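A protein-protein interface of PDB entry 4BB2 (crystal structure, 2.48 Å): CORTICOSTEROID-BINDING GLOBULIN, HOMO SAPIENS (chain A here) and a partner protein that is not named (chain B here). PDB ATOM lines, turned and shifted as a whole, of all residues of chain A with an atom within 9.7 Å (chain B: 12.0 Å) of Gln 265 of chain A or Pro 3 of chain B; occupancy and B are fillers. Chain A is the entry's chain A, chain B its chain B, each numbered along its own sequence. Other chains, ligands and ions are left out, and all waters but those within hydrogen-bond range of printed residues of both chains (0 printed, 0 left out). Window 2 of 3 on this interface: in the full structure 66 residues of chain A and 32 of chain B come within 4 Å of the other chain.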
ATOM      1  N   GLN A 178     -19.926  -9.092   7.776  1.00  0.00           N
ATOM      2  CA  GLN A 178     -18.950  -9.452   6.751  1.00  0.00           C
ATOM      3  C   GLN A 178     -17.908  -8.348   6.599  1.00  0.00           C
ATOM      4  O   GLN A 178     -18.094  -7.419   5.815  1.00  0.00           O
ATOM      5  CB  GLN A 178     -19.644  -9.688   5.409  1.00  0.00           C
ATOM      6  CG  GLN A 178     -20.594 -10.873   5.394  1.00  0.00           C
ATOM      7  CD  GLN A 178     -21.084 -11.210   3.993  1.00  0.00           C
ATOM      8  OE1 GLN A 178     -20.416 -10.915   2.993  1.00  0.00           O
ATOM      9  NE2 GLN A 178     -22.253 -11.841   3.915  1.00  0.00           N
ATOM     10  N   LEU A 204     -12.238  -3.250  -0.046  1.00  0.00           N
ATOM     11  CA  LEU A 204     -12.703  -4.355  -0.871  1.00  0.00           C
ATOM     12  C   LEU A 204     -13.117  -5.552  -0.030  1.00  0.00           C
ATOM     13  O   LEU A 204     -12.506  -5.838   0.995  1.00  0.00           O
ATOM     14  CB  LEU A 204     -11.613  -4.778  -1.856  1.00  0.00           C
ATOM     15  CG  LEU A 204     -11.713  -6.114  -2.611  1.00  0.00           C
ATOM     16  CD1 LEU A 204     -12.941  -6.157  -3.526  1.00  0.00           C
ATOM     17  CD2 LEU A 204     -10.446  -6.356  -3.414  1.00  0.00           C
ATOM     18  N   GLN A 205     -14.173  -6.231  -0.474  1.00  0.00           N
ATOM     19  CA  GLN A 205     -14.417  -7.620  -0.119  1.00  0.00           C
ATOM     20  C   GLN A 205     -15.000  -8.392  -1.316  1.00  0.00           C
ATOM     21  O   GLN A 205     -15.726  -7.826  -2.132  1.00  0.00           O
ATOM     22  CB  GLN A 205     -15.306  -7.728   1.116  1.00  0.00           C
ATOM     23  CG  GLN A 205     -16.782  -7.383   0.940  1.00  0.00           C
ATOM     24  CD  GLN A 205     -17.559  -7.721   2.198  1.00  0.00           C
ATOM     25  OE1 GLN A 205     -18.103  -8.813   2.315  1.00  0.00           O
ATOM     26  NE2 GLN A 205     -17.569  -6.805   3.172  1.00  0.00           N
ATOM     27  N   SER A 206     -14.651  -9.670  -1.432  1.00  0.00           N
ATOM     28  CA  SER A 206     -15.271 -10.556  -2.427  1.00  0.00           C
ATOM     29  C   SER A 206     -16.047 -11.623  -1.696  1.00  0.00           C
ATOM     30  O   SER A 206     -15.455 -12.515  -1.084  1.00  0.00           O
ATOM     31  CB  SER A 206     -14.217 -11.217  -3.304  1.00  0.00           C
ATOM     32  OG  SER A 206     -13.422 -10.230  -3.922  1.00  0.00           O
ATOM     33  N   SER A 207     -17.369 -11.538  -1.740  1.00  0.00           N
ATOM     34  CA  SER A 207     -18.192 -12.461  -0.968  1.00  0.00           C
ATOM     35  C   SER A 207     -19.633 -12.519  -1.435  1.00  0.00           C
ATOM     36  O   SER A 207     -19.984 -11.941  -2.454  1.00  0.00           O
ATOM     37  CB  SER A 207     -18.112 -12.134   0.533  1.00  0.00           C
ATOM     38  OG  SER A 207     -18.256 -10.746   0.771  1.00  0.00           O
ATOM     39  N   THR A 208     -20.451 -13.266  -0.705  1.00  0.00           N
ATOM     40  CA  THR A 208     -21.860 -13.342  -1.004  1.00  0.00           C
ATOM     41  C   THR A 208     -22.515 -12.128  -0.377  1.00  0.00           C
ATOM     42  O   THR A 208     -22.452 -11.930   0.834  1.00  0.00           O
ATOM     43  CB  THR A 208     -22.482 -14.653  -0.488  1.00  0.00           C
ATOM     44  OG1 THR A 208     -21.835 -15.756  -1.132  1.00  0.00           O
ATOM     45  CG2 THR A 208     -23.981 -14.712  -0.811  1.00  0.00           C
ATOM     46  N   ILE A 209     -23.117 -11.303  -1.222  1.00  0.00           N
ATOM     47  CA  ILE A 209     -23.724 -10.054  -0.789  1.00  0.00           C
ATOM     48  C   ILE A 209     -25.103  -9.861  -1.426  1.00  0.00           C
ATOM     49  O   ILE A 209     -25.323 -10.278  -2.568  1.00  0.00           O
ATOM     50  CB  ILE A 209     -22.740  -8.887  -1.017  1.00  0.00           C
ATOM     51  CG1 ILE A 209     -21.845  -8.775   0.223  1.00  0.00           C
ATOM     52  CG2 ILE A 209     -23.454  -7.558  -1.232  1.00  0.00           C
ATOM     53  CD1 ILE A 209     -20.441  -8.301  -0.058  1.00  0.00           C
ATOM     54  N   SER A 210     -26.041  -9.292  -0.663  1.00  0.00           N
ATOM     55  CA  SER A 210     -27.368  -8.944  -1.192  1.00  0.00           C
ATOM     56  C   SER A 210     -27.290  -7.779  -2.165  1.00  0.00           C
ATOM     57  O   SER A 210     -26.971  -6.663  -1.778  1.00  0.00           O
ATOM     58  CB  SER A 210     -28.333  -8.622  -0.067  1.00  0.00           C
ATOM     59  OG  SER A 210     -28.586  -9.792   0.671  1.00  0.00           O
ATOM     60  N   TYR A 211     -27.575  -8.067  -3.430  1.00  0.00           N
ATOM     61  CA  TYR A 211     -27.354  -7.121  -4.509  1.00  0.00           C
ATOM     62  C   TYR A 211     -28.596  -6.983  -5.369  1.00  0.00           C
ATOM     63  O   TYR A 211     -29.358  -7.938  -5.533  1.00  0.00           O
ATOM     64  CB  TYR A 211     -26.183  -7.584  -5.388  1.00  0.00           C
ATOM     65  CG  TYR A 211     -26.043  -6.831  -6.705  1.00  0.00           C
ATOM     66  CD1 TYR A 211     -25.336  -5.630  -6.768  1.00  0.00           C
ATOM     67  CD2 TYR A 211     -26.615  -7.319  -7.891  1.00  0.00           C
ATOM     68  CE1 TYR A 211     -25.194  -4.939  -7.967  1.00  0.00           C
ATOM     69  CE2 TYR A 211     -26.482  -6.632  -9.094  1.00  0.00           C
ATOM     70  CZ  TYR A 211     -25.769  -5.446  -9.120  1.00  0.00           C
ATOM     71  OH  TYR A 211     -25.617  -4.749 -10.286  1.00  0.00           O
ATOM     72  N   LEU A 212     -28.786  -5.788  -5.916  1.00  0.00           N
ATOM     73  CA  LEU A 212     -29.842  -5.548  -6.875  1.00  0.00           C
ATOM     74  C   LEU A 212     -29.426  -4.462  -7.850  1.00  0.00           C
ATOM     75  O   LEU A 212     -29.093  -3.345  -7.440  1.00  0.00           O
ATOM     76  CB  LEU A 212     -31.152  -5.157  -6.185  1.00  0.00           C
ATOM     77  CG  LEU A 212     -32.317  -4.726  -7.105  1.00  0.00           C
ATOM     78  CD1 LEU A 212     -32.796  -5.852  -8.022  1.00  0.00           C
ATOM     79  CD2 LEU A 212     -33.467  -4.176  -6.279  1.00  0.00           C
ATOM     80  N   VAL A 222     -26.625  -2.497  -2.648  1.00  0.00           N
ATOM     81  CA  VAL A 222     -26.418  -3.652  -1.805  1.00  0.00           C
ATOM     82  C   VAL A 222     -27.003  -3.404  -0.425  1.00  0.00           C
ATOM     83  O   VAL A 222     -27.195  -2.250  -0.010  1.00  0.00           O
ATOM     84  CB  VAL A 222     -24.927  -4.060  -1.707  1.00  0.00           C
ATOM     85  CG1 VAL A 222     -24.386  -4.406  -3.089  1.00  0.00           C
ATOM     86  CG2 VAL A 222     -24.103  -2.964  -1.044  1.00  0.00           C
ATOM     87  N   THR A 262     -30.901 -10.033  -4.164  1.00  0.00           N
ATOM     88  CA  THR A 262     -30.515 -11.435  -4.317  1.00  0.00           C
ATOM     89  C   THR A 262     -29.070 -11.620  -3.893  1.00  0.00           C
ATOM     90  O   THR A 262     -28.203 -10.819  -4.263  1.00  0.00           O
ATOM     91  CB  THR A 262     -30.659 -11.897  -5.791  1.00  0.00           C
ATOM     92  OG1 THR A 262     -32.014 -11.749  -6.204  1.00  0.00           O
ATOM     93  CG2 THR A 262     -30.274 -13.368  -5.980  1.00  0.00           C
ATOM     94  N   SER A 263     -28.826 -12.678  -3.120  1.00  0.00           N
ATOM     95  CA  SER A 263     -27.476 -13.110  -2.767  1.00  0.00           C
ATOM     96  C   SER A 263     -26.681 -13.330  -4.038  1.00  0.00           C
ATOM     97  O   SER A 263     -27.086 -14.113  -4.892  1.00  0.00           O
ATOM     98  CB  SER A 263     -27.523 -14.416  -1.969  1.00  0.00           C
ATOM     99  OG  SER A 263     -28.231 -14.258  -0.754  1.00  0.00           O
ATOM    100  N   SER A 264     -25.563 -12.622  -4.175  1.00  0.00           N
ATOM    101  CA  SER A 264     -24.743 -12.711  -5.387  1.00  0.00           C
ATOM    102  C   SER A 264     -23.259 -12.579  -5.072  1.00  0.00           C
ATOM    103  O   SER A 264     -22.889 -11.942  -4.080  1.00  0.00           O
ATOM    104  CB  SER A 264     -25.140 -11.624  -6.384  1.00  0.00           C
ATOM    105  OG  SER A 264     -26.527 -11.349  -6.318  1.00  0.00           O
ATOM    106  N   GLN A 265     -22.418 -13.174  -5.919  1.00  0.00           N
ATOM    107  CA  GLN A 265     -20.972 -12.952  -5.857  1.00  0.00           C
ATOM    108  C   GLN A 265     -20.671 -11.552  -6.368  1.00  0.00           C
ATOM    109  O   GLN A 265     -20.957 -11.216  -7.522  1.00  0.00           O
ATOM    110  CB  GLN A 265     -20.185 -14.002  -6.655  1.00  0.00           C
ATOM    111  CG  GLN A 265     -20.459 -15.444  -6.254  1.00  0.00           C
ATOM    112  CD  GLN A 265     -20.517 -15.638  -4.746  1.00  0.00           C
ATOM    113  OE1 GLN A 265     -19.522 -15.439  -4.030  1.00  0.00           O
ATOM    114  NE2 GLN A 265     -21.686 -16.037  -4.253  1.00  0.00           N
ATOM    115  N   VAL A 266     -20.110 -10.736  -5.481  1.00  0.00           N
ATOM    116  CA  VAL A 266     -19.845  -9.340  -5.759  1.00  0.00           C
ATOM    117  C   VAL A 266     -18.443  -8.996  -5.273  1.00  0.00           C
ATOM    118  O   VAL A 266     -18.103  -9.270  -4.113  1.00  0.00           O
ATOM    119  CB  VAL A 266     -20.855  -8.405  -5.033  1.00  0.00           C
ATOM    120  CG1 VAL A 266     -20.468  -6.943  -5.215  1.00  0.00           C
ATOM    121  CG2 VAL A 266     -22.283  -8.643  -5.505  1.00  0.00           C
ATOM    122  N   ASP A 267     -17.640  -8.406  -6.161  1.00  0.00           N
ATOM    123  CA  ASP A 267     -16.448  -7.674  -5.746  1.00  0.00           C
ATOM    124  C   ASP A 267     -16.902  -6.296  -5.296  1.00  0.00           C
ATOM    125  O   ASP A 267     -17.264  -5.452  -6.115  1.00  0.00           O
ATOM    126  CB  ASP A 267     -15.420  -7.591  -6.878  1.00  0.00           C
ATOM    127  CG  ASP A 267     -14.680  -8.908  -7.088  1.00  0.00           C
ATOM    128  OD1 ASP A 267     -14.731  -9.772  -6.185  1.00  0.00           O
ATOM    129  OD2 ASP A 267     -14.038  -9.086  -8.147  1.00  0.00           O
ATOM    130  N   LEU A 268     -16.936  -6.094  -3.985  1.00  0.00           N
ATOM    131  CA  LEU A 268     -17.522  -4.897  -3.416  1.00  0.00           C
ATOM    132  C   LEU A 268     -16.488  -3.900  -2.943  1.00  0.00           C
ATOM    133  O   LEU A 268     -15.766  -4.149  -1.961  1.00  0.00           O
ATOM    134  CB  LEU A 268     -18.467  -5.260  -2.284  1.00  0.00           C
ATOM    135  CG  LEU A 268     -19.194  -4.093  -1.622  1.00  0.00           C
ATOM    136  CD1 LEU A 268     -20.207  -3.444  -2.557  1.00  0.00           C
ATOM    137  CD2 LEU A 268     -19.849  -4.599  -0.343  1.00  0.00           C
ATOM    138  N   TYR A 269     -16.412  -2.783  -3.666  1.00  0.00           N
ATOM    139  CA  TYR A 269     -15.508  -1.685  -3.361  1.00  0.00           C
ATOM    140  C   TYR A 269     -16.313  -0.541  -2.774  1.00  0.00           C
ATOM    141  O   TYR A 269     -17.213   0.013  -3.426  1.00  0.00           O
ATOM    142  CB  TYR A 269     -14.779  -1.202  -4.619  1.00  0.00           C
ATOM    143  CG  TYR A 269     -13.913  -2.238  -5.299  1.00  0.00           C
ATOM    144  CD1 TYR A 269     -14.456  -3.127  -6.241  1.00  0.00           C
ATOM    145  CD2 TYR A 269     -12.550  -2.323  -5.018  1.00  0.00           C
ATOM    146  CE1 TYR A 269     -13.661  -4.080  -6.877  1.00  0.00           C
ATOM    147  CE2 TYR A 269     -11.742  -3.271  -5.645  1.00  0.00           C
ATOM    148  CZ  TYR A 269     -12.300  -4.147  -6.569  1.00  0.00           C
ATOM    149  OH  TYR A 269     -11.503  -5.088  -7.191  1.00  0.00           O
ATOM    150  N   LYS B   2     -19.171 -15.584 -12.807  1.00  0.00           N
ATOM    151  CA  LYS B   2     -18.335 -14.391 -12.839  1.00  0.00           C
ATOM    152  C   LYS B   2     -18.885 -13.306 -11.917  1.00  0.00           C
ATOM    153  O   LYS B   2     -19.998 -12.806 -12.133  1.00  0.00           O
ATOM    154  CB  LYS B   2     -18.181 -13.862 -14.271  1.00  0.00           C
ATOM    155  CG  LYS B   2     -16.990 -14.443 -15.021  1.00  0.00           C
ATOM    156  CD  LYS B   2     -17.291 -15.811 -15.620  1.00  0.00           C
ATOM    157  CE  LYS B   2     -16.019 -16.623 -15.817  1.00  0.00           C
ATOM    158  NZ  LYS B   2     -15.018 -15.937 -16.682  1.00  0.00           N
ATOM    159  N   PRO B   3     -18.103 -12.944 -10.878  1.00  0.00           N
ATOM    160  CA  PRO B   3     -18.522 -11.976  -9.852  1.00  0.00           C
ATOM    161  C   PRO B   3     -18.911 -10.614 -10.426  1.00  0.00           C
ATOM    162  O   PRO B   3     -18.291 -10.136 -11.389  1.00  0.00           O
ATOM    163  CB  PRO B   3     -17.275 -11.829  -8.956  1.00  0.00           C
ATOM    164  CG  PRO B   3     -16.141 -12.429  -9.728  1.00  0.00           C
ATOM    165  CD  PRO B   3     -16.751 -13.476 -10.616  1.00  0.00           C
ATOM    166  N   ILE B   4     -19.933 -10.007  -9.830  1.00  0.00           N
ATOM    167  CA  ILE B   4     -20.343  -8.652 -10.166  1.00  0.00           C
ATOM    168  C   ILE B   4     -19.332  -7.692  -9.551  1.00  0.00           C
ATOM    169  O   ILE B   4     -19.023  -7.796  -8.368  1.00  0.00           O
ATOM    170  CB  ILE B   4     -21.762  -8.355  -9.624  1.00  0.00           C
ATOM    171  CG1 ILE B   4     -22.796  -9.265 -10.304  1.00  0.00           C
ATOM    172  CG2 ILE B   4     -22.130  -6.892  -9.826  1.00  0.00           C
ATOM    173  CD1 ILE B   4     -24.033  -9.527  -9.472  1.00  0.00           C
ATOM    174  N   ILE B   5     -18.805  -6.775 -10.355  1.00  0.00           N
ATOM    175  CA  ILE B   5     -17.900  -5.750  -9.841  1.00  0.00           C
ATOM    176  C   ILE B   5     -18.679  -4.466  -9.527  1.00  0.00           C
ATOM    177  O   ILE B   5     -19.202  -3.814 -10.431  1.00  0.00           O
ATOM    178  CB  ILE B   5     -16.745  -5.456 -10.825  1.00  0.00           C
ATOM    179  CG1 ILE B   5     -15.895  -6.720 -11.048  1.00  0.00           C
ATOM    180  CG2 ILE B   5     -15.903  -4.282 -10.326  1.00  0.00           C
ATOM    181  CD1 ILE B   5     -14.835  -6.596 -12.126  1.00  0.00           C
ATOM    182  N   LEU B   6     -18.736  -4.102  -8.249  1.00  0.00           N
ATOM    183  CA  LEU B   6     -19.464  -2.912  -7.831  1.00  0.00           C
ATOM    184  C   LEU B   6     -18.563  -1.914  -7.114  1.00  0.00           C
ATOM    185  O   LEU B   6     -18.175  -2.147  -5.971  1.00  0.00           O
ATOM    186  CB  LEU B   6     -20.628  -3.304  -6.915  1.00  0.00           C
ATOM    187  CG  LEU B   6     -21.624  -2.202  -6.574  1.00  0.00           C
ATOM    188  CD1 LEU B   6     -22.321  -1.686  -7.834  1.00  0.00           C
ATOM    189  CD2 LEU B   6     -22.632  -2.727  -5.578  1.00  0.00           C
ATOM    190  N   ARG B   7     -18.263  -0.798  -7.782  1.00  0.00           N
ATOM    191  CA  ARG B   7     -17.378   0.225  -7.227  1.00  0.00           C
ATOM    192  C   ARG B   7     -18.155   1.472  -6.783  1.00  0.00           C
ATOM    193  O   ARG B   7     -18.758   2.178  -7.604  1.00  0.00           O
ATOM    194  CB  ARG B   7     -16.264   0.611  -8.223  1.00  0.00           C
ATOM    195  CG  ARG B   7     -15.769  -0.514  -9.130  1.00  0.00           C
ATOM    196  CD  ARG B   7     -14.259  -0.460  -9.355  1.00  0.00           C
ATOM    197  NE  ARG B   7     -13.849   0.472 -10.404  1.00  0.00           N
ATOM    198  CZ  ARG B   7     -14.625   0.856 -11.405  1.00  0.00           C
ATOM    199  NH1 ARG B   7     -15.860   0.385 -11.502  1.00  0.00           N
ATOM    200  NH2 ARG B   7     -14.164   1.709 -12.310  1.00  0.00           N
ATOM    201  N   PHE B   8     -18.137   1.745  -5.482  1.00  0.00           N
ATOM    202  CA  PHE B   8     -18.737   2.971  -4.968  1.00  0.00           C
ATOM    203  C   PHE B   8     -17.722   4.110  -5.082  1.00  0.00           C
ATOM    204  O   PHE B   8     -17.279   4.661  -4.078  1.00  0.00           O
ATOM    205  CB  PHE B   8     -19.242   2.794  -3.530  1.00  0.00           C
ATOM    206  CG  PHE B   8     -20.535   2.031  -3.430  1.00  0.00           C
ATOM    207  CD1 PHE B   8     -20.554   0.639  -3.543  1.00  0.00           C
ATOM    208  CD2 PHE B   8     -21.748   2.705  -3.245  1.00  0.00           C
ATOM    209  CE1 PHE B   8     -21.754  -0.064  -3.454  1.00  0.00           C
ATOM    210  CE2 PHE B   8     -22.946   2.010  -3.159  1.00  0.00           C
ATOM    211  CZ  PHE B   8     -22.950   0.624  -3.261  1.00  0.00           C
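O of Gln 205 of chain A is in hydrogen-bond range of N of Leu 268 of chain A (2.8 Å). The side-chain hydroxyl of Ser 206 of chain A is in hydrogen-bond range of the side-chain carboxylate of Asp 267 of chain A (2.7 Å). NE2 of Gln 265 of chain A is in hydrogen-bond range of OG1 of Thr 208 of chain A (3.1 Å). The backbone carbonyl oxygen of Ile 209 of chain A is in hydrogen-bond range of the backbone NH of Ser 264 of chain A, at 2.9 Å. The backbone NH (N) of Thr 262 of chain A is in hydrogen-bond range of the backbone carbonyl oxygen (O) of Tyr 211 of chain A (2.9 Å). The backbone carbonyl oxygen (O) of Thr 262 of chain A sits at hydrogen-bond distance from the side-chain hydroxyl (OG) of Ser 264 of chain A (2.7 Å).
Tyr 211 of chain A touches Ile 4 of chain B (CD2 to CD1, 3.7 Å). Leu 6 of chain B touches Val 222 of chain A. Ile 4 of chain B touches Ser 264 of chain A (CD1 to CB, 3.9 Å). Gln 265 of chain A touches Pro 3 of chain B (O to CA, 3.5 Å). Ile 4 of chain B touches Val 266 of chain A (O to CA, 3.1 Å). Ile 5 of chain B touches Asp 267 of chain A (CA to O, 3.8 Å). Leu 268 of chain A touches Leu 6 of chain B (CA to O, 3.8 Å). Leu 268 of chain A touches Phe 8 of chain B (CD1 to CE1, 3.8 Å). C of Arg 7 of chain B touches O of Tyr 269 of chain A, 3.8 Å away.
Of the 7 printed residues of chain B, 6 touch a printed residue of chain A. Hydrophobic or aromatic side chains of chain B within 4 Å of the printed part of chain A: Pro 3, Ile 4, Leu 6 and Phe 8. Among the printed residues, no Asp or Glu carboxylate lies within 4 Å of a Lys or Arg side-chain nitrogen of the other chain.
N of Ile 4 of chain B lies within hydrogen-bond range of O of Gln 265 of chain A, at 2.8 Å. O of Ile 4 of chain B lies within hydrogen-bond range of N of Asp 267 of chain A. The backbone carbonyl oxygen (O) of Asp 267 of chain A sits at hydrogen-bond distance from the backbone NH (N) of Leu 6 of chain B, at 2.9 Å. The backbone carbonyl oxygen (O) of Leu 6 of chain B sits at hydrogen-bond distance from the backbone NH (N) of Tyr 269 of chain A (3.0 Å). The backbone NH (N) of Phe 8 of chain B lies within hydrogen-bond range of the backbone carbonyl oxygen (O) of Tyr 269 of chain A.
Leu 204 of chain A touches none of the printed residues of chain B. Ser 207 of chain A touches none of the printed residues of chain B. No residue of chain B comes within 4 Å of Thr 208 of chain A. No residue of chain B comes within 4 Å of Ile 209 of chain A. Of the printed residues of chain B, Val 222 of chain A touches Leu 6. Ser 264 of chain A touches just one residue of chain B: Ile 4 (3.9 Å). Of chain B, only Pro 3 (3.5 Å) and Ile 4 (2.8 Å) come within 4 Å of Gln 265 of chain A. Of the printed residues of chain B, Val 266 of chain A touches Ile 4 (3.1 Å). Of chain B, only Ile 4 (2.7 Å), Ile 5 (3.8 Å) and Leu 6 (2.9 Å) come within 4 Å of Asp 267 of chain A. Printed residues of chain B within 4 Å of Leu 268 of chain A: Leu 6 and Phe 8. Printed residues of chain A within 4 Å of Pro 3 of chain B: Gln 265. Of chain A, only Tyr 211, Ser 264, Gln 265, Val 266 and Asp 267 come within 4 Å of Ile 4 of chain B. Of the printed residues of chain A, Leu 6 of chain B touches Val 222 (3.5 Å), Asp 267 (2.9 Å), Leu 268 (3.8 Å) and Tyr 269 (3.0 Å). Printed residues of chain A within 4 Å of Arg 7 of chain B: Tyr 269. The nearest residue of chain A that does not touch Pro 3 of chain B is Asp 267 of chain A (4.3 Å). The nearest printed residue of chain A that does not touch Leu 6 of chain B is Val 266 of chain A (4.02 Å).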
